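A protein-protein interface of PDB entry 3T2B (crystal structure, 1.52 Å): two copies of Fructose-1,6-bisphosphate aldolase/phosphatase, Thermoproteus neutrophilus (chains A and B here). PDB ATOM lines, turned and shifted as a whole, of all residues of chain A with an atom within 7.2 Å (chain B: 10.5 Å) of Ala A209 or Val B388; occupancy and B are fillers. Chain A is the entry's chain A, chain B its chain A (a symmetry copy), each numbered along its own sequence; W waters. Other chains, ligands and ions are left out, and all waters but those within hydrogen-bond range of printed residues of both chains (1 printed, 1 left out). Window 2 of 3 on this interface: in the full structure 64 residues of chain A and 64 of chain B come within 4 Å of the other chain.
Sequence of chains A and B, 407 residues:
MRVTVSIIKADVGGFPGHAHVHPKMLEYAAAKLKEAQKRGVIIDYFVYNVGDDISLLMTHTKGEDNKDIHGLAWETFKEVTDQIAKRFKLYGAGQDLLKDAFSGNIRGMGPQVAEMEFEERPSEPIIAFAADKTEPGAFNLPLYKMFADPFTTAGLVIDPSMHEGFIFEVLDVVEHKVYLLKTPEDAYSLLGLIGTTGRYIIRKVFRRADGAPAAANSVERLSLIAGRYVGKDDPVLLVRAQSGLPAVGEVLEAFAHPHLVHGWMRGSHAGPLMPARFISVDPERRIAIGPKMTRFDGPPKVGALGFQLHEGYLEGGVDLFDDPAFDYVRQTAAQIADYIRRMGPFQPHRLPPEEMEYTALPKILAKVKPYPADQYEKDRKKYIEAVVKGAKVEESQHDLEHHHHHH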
ATOM      1  N   SER A 161      14.919 -13.682  11.704  1.00  0.00           N
ATOM      2  CA  SER A 161      14.522 -12.719  12.750  1.00  0.00           C
ATOM      3  C   SER A 161      15.678 -11.908  13.326  1.00  0.00           C
ATOM      4  O   SER A 161      15.463 -10.953  14.044  1.00  0.00           O
ATOM      5  CB  SER A 161      13.743 -13.343  13.891  1.00  0.00           C
ATOM      6  OG  SER A 161      14.602 -14.116  14.785  1.00  0.00           O
ATOM      7  N   MET A 162      16.915 -12.334  13.016  1.00  0.00           N
ATOM      8  CA  MET A 162      18.086 -11.649  13.555  1.00  0.00           C
ATOM      9  C   MET A 162      18.859 -10.854  12.546  1.00  0.00           C
ATOM     10  O   MET A 162      19.907 -10.198  12.903  1.00  0.00           O
ATOM     11  CB  MET A 162      19.038 -12.726  14.192  1.00  0.00           C
ATOM     12  CG  MET A 162      18.413 -13.295  15.345  1.00  0.00           C
ATOM     13  SD  MET A 162      19.431 -14.593  16.171  1.00  0.00           S
ATOM     14  CE  MET A 162      20.637 -13.512  16.952  1.00  0.00           C
ATOM     15  N   GLU A 164      18.631  -8.030  11.057  1.00  0.00           N
ATOM     16  CA  GLU A 164      18.821  -6.601  11.221  1.00  0.00           C
ATOM     17  C   GLU A 164      19.839  -6.227  12.267  1.00  0.00           C
ATOM     18  O   GLU A 164      20.118  -5.058  12.467  1.00  0.00           O
ATOM     19  CB  GLU A 164      17.442  -5.928  11.482  1.00  0.00           C
ATOM     20  CG  GLU A 164      16.605  -5.846  10.160  1.00  0.00           C
ATOM     21  CD  GLU A 164      15.842  -7.127   9.787  1.00  0.00           C
ATOM     22  OE1 GLU A 164      15.132  -7.670  10.688  1.00  0.00           O
ATOM     23  OE2 GLU A 164      15.909  -7.567   8.588  1.00  0.00           O
ATOM     24  N   GLY A 165      20.244  -7.198  13.077  1.00  0.00           N
ATOM     25  CA  GLY A 165      21.356  -6.918  13.979  1.00  0.00           C
ATOM     26  C   GLY A 165      20.986  -6.225  15.256  1.00  0.00           C
ATOM     27  O   GLY A 165      19.841  -6.314  15.782  1.00  0.00           O
ATOM     28  N   PHE A 166      21.975  -5.546  15.845  1.00  0.00           N
ATOM     29  CA  PHE A 166      21.878  -5.072  17.187  1.00  0.00           C
ATOM     30  C   PHE A 166      22.435  -3.665  17.384  1.00  0.00           C
ATOM     31  O   PHE A 166      23.190  -3.213  16.539  1.00  0.00           O
ATOM     32  CB  PHE A 166      22.616  -6.096  18.197  1.00  0.00           C
ATOM     33  CG  PHE A 166      21.832  -7.366  18.324  1.00  0.00           C
ATOM     34  CD1 PHE A 166      22.023  -8.442  17.375  1.00  0.00           C
ATOM     35  CD2 PHE A 166      20.851  -7.493  19.331  1.00  0.00           C
ATOM     36  CE1 PHE A 166      21.263  -9.606  17.453  1.00  0.00           C
ATOM     37  CE2 PHE A 166      20.049  -8.614  19.332  1.00  0.00           C
ATOM     38  CZ  PHE A 166      20.245  -9.649  18.400  1.00  0.00           C
ATOM     39  N   ILE A 167      21.969  -3.024  18.465  1.00  0.00           N
ATOM     40  CA  ILE A 167      22.437  -1.667  18.878  1.00  0.00           C
ATOM     41  C   ILE A 167      23.264  -1.821  20.148  1.00  0.00           C
ATOM     42  O   ILE A 167      22.824  -2.357  21.162  1.00  0.00           O
ATOM     43  CB  ILE A 167      21.196  -0.732  19.185  1.00  0.00           C
ATOM     44  CG1 ILE A 167      20.323  -0.702  17.957  1.00  0.00           C
ATOM     45  CG2 ILE A 167      21.758   0.674  19.448  1.00  0.00           C
ATOM     46  CD1 ILE A 167      18.866  -0.172  18.324  1.00  0.00           C
ATOM     47  N   LYS A 182      25.504   0.495  15.546  1.00  0.00           N
ATOM     48  CA  LYS A 182      24.563  -0.587  15.071  1.00  0.00           C
ATOM     49  C   LYS A 182      25.299  -1.568  14.197  1.00  0.00           C
ATOM     50  O   LYS A 182      25.915  -1.165  13.206  1.00  0.00           O
ATOM     51  CB  LYS A 182      23.468   0.018  14.135  1.00  0.00           C
ATOM     52  CG  LYS A 182      22.611   0.989  14.899  1.00  0.00           C
ATOM     53  CD  LYS A 182      22.855   2.405  14.469  1.00  0.00           C
ATOM     54  CE  LYS A 182      22.277   2.611  13.125  1.00  0.00           C
ATOM     55  NZ  LYS A 182      23.320   3.389  12.406  1.00  0.00           N
ATOM     56  N   PHE A 206      20.733  -3.722  22.625  1.00  0.00           N
ATOM     57  CA  PHE A 206      19.296  -3.786  22.237  1.00  0.00           C
ATOM     58  C   PHE A 206      19.140  -4.420  20.927  1.00  0.00           C
ATOM     59  O   PHE A 206      19.912  -4.255  20.008  1.00  0.00           O
ATOM     60  CB  PHE A 206      18.765  -2.289  22.177  1.00  0.00           C
ATOM     61  CG  PHE A 206      18.901  -1.581  23.431  1.00  0.00           C
ATOM     62  CD1 PHE A 206      17.987  -1.721  24.497  1.00  0.00           C
ATOM     63  CD2 PHE A 206      20.005  -0.763  23.643  1.00  0.00           C
ATOM     64  CE1 PHE A 206      18.159  -1.019  25.738  1.00  0.00           C
ATOM     65  CE2 PHE A 206      20.196  -0.110  24.871  1.00  0.00           C
ATOM     66  CZ  PHE A 206      19.292  -0.231  25.916  1.00  0.00           C
ATOM     67  N   ARG A 207      18.003  -5.131  20.738  1.00  0.00           N
ATOM     68  CA  ARG A 207      17.657  -5.622  19.474  1.00  0.00           C
ATOM     69  C   ARG A 207      17.308  -4.476  18.486  1.00  0.00           C
ATOM     70  O   ARG A 207      16.556  -3.603  18.877  1.00  0.00           O
ATOM     71  CB  ARG A 207      16.517  -6.723  19.675  1.00  0.00           C
ATOM     72  CG  ARG A 207      16.128  -7.094  18.349  1.00  0.00           C
ATOM     73  CD  ARG A 207      16.068  -8.442  18.110  1.00  0.00           C
ATOM     74  NE  ARG A 207      14.807  -8.907  18.523  1.00  0.00           N
ATOM     75  CZ  ARG A 207      13.858  -9.424  17.728  1.00  0.00           C
ATOM     76  NH1 ARG A 207      13.970  -9.549  16.416  1.00  0.00           N
ATOM     77  NH2 ARG A 207      12.745  -9.860  18.320  1.00  0.00           N
ATOM     78  N   ARG A 208      17.830  -4.453  17.267  1.00  0.00           N
ATOM     79  CA  ARG A 208      17.557  -3.353  16.357  1.00  0.00           C
ATOM     80  C   ARG A 208      16.139  -3.408  15.797  1.00  0.00           C
ATOM     81  O   ARG A 208      15.557  -2.302  15.563  1.00  0.00           O
ATOM     82  CB  ARG A 208      18.503  -3.351  15.188  1.00  0.00           C
ATOM     83  CG  ARG A 208      18.676  -1.861  14.768  1.00  0.00           C
ATOM     84  CD  ARG A 208      18.773  -1.728  13.350  1.00  0.00           C
ATOM     85  NE  ARG A 208      20.069  -2.217  12.954  1.00  0.00           N
ATOM     86  CZ  ARG A 208      20.900  -1.636  12.132  1.00  0.00           C
ATOM     87  NH1 ARG A 208      20.578  -0.520  11.556  1.00  0.00           N
ATOM     88  NH2 ARG A 208      22.052  -2.265  11.836  1.00  0.00           N
ATOM     89  N   ALA A 209      15.588  -4.599  15.662  1.00  0.00           N
ATOM     90  CA  ALA A 209      14.201  -4.736  15.037  1.00  0.00           C
ATOM     91  C   ALA A 209      13.161  -3.940  15.861  1.00  0.00           C
ATOM     92  O   ALA A 209      12.264  -3.303  15.272  1.00  0.00           O
ATOM     93  CB  ALA A 209      13.780  -6.190  14.954  1.00  0.00           C
ATOM     94  N   ASP A 210      13.219  -4.020  17.182  1.00  0.00           N
ATOM     95  CA  ASP A 210      12.193  -3.500  18.040  1.00  0.00           C
ATOM     96  C   ASP A 210      12.715  -2.728  19.256  1.00  0.00           C
ATOM     97  O   ASP A 210      11.888  -2.238  20.031  1.00  0.00           O
ATOM     98  CB  ASP A 210      11.208  -4.632  18.452  1.00  0.00           C
ATOM     99  CG  ASP A 210      11.832  -5.645  19.361  1.00  0.00           C
ATOM    100  OD1 ASP A 210      13.090  -5.584  19.521  1.00  0.00           O
ATOM    101  OD2 ASP A 210      11.127  -6.427  20.023  1.00  0.00           O
ATOM    102  N   GLY A 211      14.058  -2.606  19.456  1.00  0.00           N
ATOM    103  CA  GLY A 211      14.608  -1.879  20.581  1.00  0.00           C
ATOM    104  C   GLY A 211      14.595  -2.664  21.888  1.00  0.00           C
ATOM    105  O   GLY A 211      14.905  -2.077  22.898  1.00  0.00           O
ATOM    106  N   ALA A 212      14.258  -3.961  21.855  1.00  0.00           N
ATOM    107  CA  ALA A 212      14.119  -4.771  23.063  1.00  0.00           C
ATOM    108  C   ALA A 212      15.496  -4.887  23.761  1.00  0.00           C
ATOM    109  O   ALA A 212      16.503  -5.102  23.083  1.00  0.00           O
ATOM    110  CB  ALA A 212      13.611  -6.214  22.771  1.00  0.00           C
ATOM    111  N   TYR B 371      27.092  11.224  23.098  1.00  0.00           N
ATOM    112  CA  TYR B 371      26.100  11.819  23.959  1.00  0.00           C
ATOM    113  C   TYR B 371      26.748  12.001  25.287  1.00  0.00           C
ATOM    114  O   TYR B 371      27.209  11.045  25.913  1.00  0.00           O
ATOM    115  CB  TYR B 371      24.896  10.893  24.125  1.00  0.00           C
ATOM    116  CG  TYR B 371      24.228  10.606  22.820  1.00  0.00           C
ATOM    117  CD1 TYR B 371      23.309  11.531  22.255  1.00  0.00           C
ATOM    118  CD2 TYR B 371      24.468   9.436  22.106  1.00  0.00           C
ATOM    119  CE1 TYR B 371      22.678  11.254  21.028  1.00  0.00           C
ATOM    120  CE2 TYR B 371      23.869   9.171  20.895  1.00  0.00           C
ATOM    121  CZ  TYR B 371      22.951  10.083  20.351  1.00  0.00           C
ATOM    122  OH  TYR B 371      22.366   9.804  19.144  1.00  0.00           O
ATOM    123  N   ARG B 380      17.602   7.945  26.794  1.00  0.00           N
ATOM    124  CA  ARG B 380      17.993   6.625  26.208  1.00  0.00           C
ATOM    125  C   ARG B 380      16.828   6.035  25.376  1.00  0.00           C
ATOM    126  O   ARG B 380      16.968   5.697  24.208  1.00  0.00           O
ATOM    127  CB  ARG B 380      18.420   5.631  27.306  1.00  0.00           C
ATOM    128  CG  ARG B 380      18.592   4.156  26.708  1.00  0.00           C
ATOM    129  CD  ARG B 380      18.887   3.091  27.772  1.00  0.00           C
ATOM    130  NE  ARG B 380      20.209   3.320  28.331  1.00  0.00           N
ATOM    131  CZ  ARG B 380      20.516   3.382  29.616  1.00  0.00           C
ATOM    132  NH1 ARG B 380      19.573   3.242  30.580  1.00  0.00           N
ATOM    133  NH2 ARG B 380      21.765   3.630  29.971  1.00  0.00           N
ATOM    134  N   LYS B 381      15.660   5.965  26.001  1.00  0.00           N
ATOM    135  CA  LYS B 381      14.474   5.435  25.321  1.00  0.00           C
ATOM    136  C   LYS B 381      14.184   6.155  24.030  1.00  0.00           C
ATOM    137  O   LYS B 381      13.896   5.506  23.013  1.00  0.00           O
ATOM    138  CB  LYS B 381      13.230   5.322  26.231  1.00  0.00           C
ATOM    139  CG  LYS B 381      13.106   3.905  26.859  1.00  0.00           C
ATOM    140  CD  LYS B 381      13.566   3.787  28.353  1.00  0.00           C
ATOM    141  CE  LYS B 381      12.358   3.872  29.361  1.00  0.00           C
ATOM    142  NZ  LYS B 381      12.621   4.769  30.569  1.00  0.00           N
ATOM    143  N   LYS B 382      14.330   7.471  23.986  1.00  0.00           N
ATOM    144  CA  LYS B 382      14.033   8.070  22.693  1.00  0.00           C
ATOM    145  C   LYS B 382      15.122   7.924  21.707  1.00  0.00           C
ATOM    146  O   LYS B 382      14.842   7.862  20.474  1.00  0.00           O
ATOM    147  CB  LYS B 382      13.494   9.533  22.747  1.00  0.00           C
ATOM    148  CG  LYS B 382      14.369  10.590  23.336  1.00  0.00           C
ATOM    149  CD  LYS B 382      14.036  10.845  24.855  1.00  0.00           C
ATOM    150  CE  LYS B 382      13.190   9.699  25.478  1.00  0.00           C
ATOM    151  NZ  LYS B 382      13.754   9.079  26.699  1.00  0.00           N
ATOM    152  N   TYR B 383      16.373   7.849  22.193  1.00  0.00           N
ATOM    153  CA  TYR B 383      17.476   7.662  21.239  1.00  0.00           C
ATOM    154  C   TYR B 383      17.411   6.295  20.639  1.00  0.00           C
ATOM    155  O   TYR B 383      17.688   6.137  19.467  1.00  0.00           O
ATOM    156  CB  TYR B 383      18.832   7.855  21.895  1.00  0.00           C
ATOM    157  CG  TYR B 383      19.138   9.261  22.330  1.00  0.00           C
ATOM    158  CD1 TYR B 383      18.893  10.370  21.479  1.00  0.00           C
ATOM    159  CD2 TYR B 383      19.698   9.498  23.570  1.00  0.00           C
ATOM    160  CE1 TYR B 383      19.195  11.667  21.899  1.00  0.00           C
ATOM    161  CE2 TYR B 383      20.005  10.772  24.002  1.00  0.00           C
ATOM    162  CZ  TYR B 383      19.744  11.858  23.173  1.00  0.00           C
ATOM    163  OH  TYR B 383      20.076  13.104  23.654  1.00  0.00           O
ATOM    164  N   ILE B 384      17.016   5.297  21.432  1.00  0.00           N
ATOM    165  CA  ILE B 384      16.872   3.920  20.887  1.00  0.00           C
ATOM    166  C   ILE B 384      15.670   3.814  19.966  1.00  0.00           C
ATOM    167  O   ILE B 384      15.755   3.217  18.862  1.00  0.00           O
ATOM    168  CB  ILE B 384      16.740   2.856  22.008  1.00  0.00           C
ATOM    169  CG1 ILE B 384      17.958   2.834  22.963  1.00  0.00           C
ATOM    170  CG2 ILE B 384      16.434   1.514  21.371  1.00  0.00           C
ATOM    171  CD1 ILE B 384      19.309   2.516  22.344  1.00  0.00           C
ATOM    172  N   GLU B 385      14.532   4.433  20.365  1.00  0.00           N
ATOM    173  CA  GLU B 385      13.402   4.508  19.443  1.00  0.00           C
ATOM    174  C   GLU B 385      13.760   5.161  18.126  1.00  0.00           C
ATOM    175  O   GLU B 385      13.305   4.729  17.102  1.00  0.00           O
ATOM    176  CB  GLU B 385      12.223   5.237  20.078  1.00  0.00           C
ATOM    177  CG  GLU B 385      11.272   4.313  20.825  1.00  0.00           C
ATOM    178  CD  GLU B 385      10.335   5.080  21.770  1.00  0.00           C
ATOM    179  OE1 GLU B 385      10.200   4.670  22.952  1.00  0.00           O
ATOM    180  OE2 GLU B 385       9.746   6.098  21.330  1.00  0.00           O
ATOM    181  N   ALA B 386      14.641   6.152  18.143  1.00  0.00           N
ATOM    182  CA  ALA B 386      15.046   6.830  16.923  1.00  0.00           C
ATOM    183  C   ALA B 386      15.887   5.934  16.022  1.00  0.00           C
ATOM    184  O   ALA B 386      15.599   5.819  14.816  1.00  0.00           O
ATOM    185  CB  ALA B 386      15.769   8.105  17.250  1.00  0.00           C
ATOM    186  N   VAL B 387      16.880   5.243  16.621  1.00  0.00           N
ATOM    187  CA  VAL B 387      17.683   4.265  15.865  1.00  0.00           C
ATOM    188  C   VAL B 387      16.782   3.159  15.315  1.00  0.00           C
ATOM    189  O   VAL B 387      16.937   2.735  14.164  1.00  0.00           O
ATOM    190  CB  VAL B 387      18.846   3.656  16.756  1.00  0.00           C
ATOM    191  CG1 VAL B 387      19.635   2.588  16.004  1.00  0.00           C
ATOM    192  CG2 VAL B 387      19.776   4.761  17.319  1.00  0.00           C
ATOM    193  N   VAL B 388      15.837   2.681  16.122  1.00  0.00           N
ATOM    194  CA  VAL B 388      14.922   1.653  15.680  1.00  0.00           C
ATOM    195  C   VAL B 388      14.047   2.145  14.515  1.00  0.00           C
ATOM    196  O   VAL B 388      13.880   1.432  13.523  1.00  0.00           O
ATOM    197  CB  VAL B 388      14.034   1.135  16.851  1.00  0.00           C
ATOM    198  CG1 VAL B 388      12.942   0.168  16.346  1.00  0.00           C
ATOM    199  CG2 VAL B 388      14.902   0.417  17.885  1.00  0.00           C
ATOM    200  N   LYS B 389      13.490   3.361  14.646  1.00  0.00           N
ATOM    201  CA  LYS B 389      12.649   3.967  13.572  1.00  0.00           C
ATOM    202  C   LYS B 389      13.482   4.796  12.608  1.00  0.00           C
ATOM    203  O   LYS B 389      13.977   4.257  11.617  1.00  0.00           O
ATOM    204  CB  LYS B 389      11.518   4.799  14.174  1.00  0.00           C
ATOM    205  CG  LYS B 389      10.738   4.032  15.302  1.00  0.00           C
ATOM    206  CD  LYS B 389       9.428   4.731  15.699  1.00  0.00           C
ATOM    207  CE  LYS B 389       9.058   4.498  17.166  1.00  0.00           C
ATOM    208  NZ  LYS B 389       8.074   5.555  17.557  1.00  0.00           N
HETATM  209  O   HOH W   1      15.156  -1.107  13.257  1.00  0.00           O
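Among the printed residues, pairs that only touch across the chains: Ile A167 with Val B387, Lys A182 with Val B387, Phe A206 with Arg B380, Phe A206 with Ile B384, Arg A208 with Val B388, Ala A209 with Val B388, Gly A211 with Ile B384 and Gly A211 with Val B388.
Water W1 lies within hydrogen-bond range of the backbone carbonyl oxygen (O) of Arg A208 (2.6 Å) and the backbone carbonyl oxygen (O) of Val B388 (2.9 Å).
No residue of chain B comes within 4 Å of Gly A165. Of the printed residues of chain B, Ile A167 touches Val B387. Printed residues of chain B within 4 Å of Lys A182: Val B387. Of the printed residues of chain B, Arg A208 touches Val B388. Ala A209 touches just one residue of chain B: Val B388 (3.7 Å). Printed residues of chain A within 4 Å of Arg B380: Phe A206. Of the printed residues of chain A, Val B387 touches Ile A167 and Lys A182. Of chain A, only Arg A208 (3.6 Å), Ala A209 (3.7 Å) and Gly A211 (3.5 Å) come within 4 Å of Val B388. The nearest residue of chain A that does not touch Val B388 is Ile A167 (4.03 Å). The nearest printed residue of chain B that does not touch Lys A182 is Val B388 (7.1 Å).
No position is printed for both chains. Of the 8 pairs that touch across the chains among the printed residues, none has its exchanged pair printed and touching as well.
NE of Arg A208 is in hydrogen-bond range of O of Glu A164 (2.9 Å). O of Gly A165 sits at hydrogen-bond distance from N of Arg A208 (3.1 Å). The backbone NH (N) of Ile A167 lies within hydrogen-bond range of the backbone carbonyl oxygen (O) of Phe A206, 2.9 Å away.
Hydrophobic or aromatic side chains of chain A that line the printed part of chain B: Ile A167 and Phe A206. Of the 11 printed residues of chain B, 4 touch a printed residue of chain A. Printed residues of chain B that touch a printed residue of chain A: Arg B380, Ile B384, Val B387 and Val B388. Hydrophobic or aromatic side chains of chain B that line the printed part of chain A: Ile B384, Val B387 and Val B388. Among the printed residues, 8 pairs touch across the chains.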
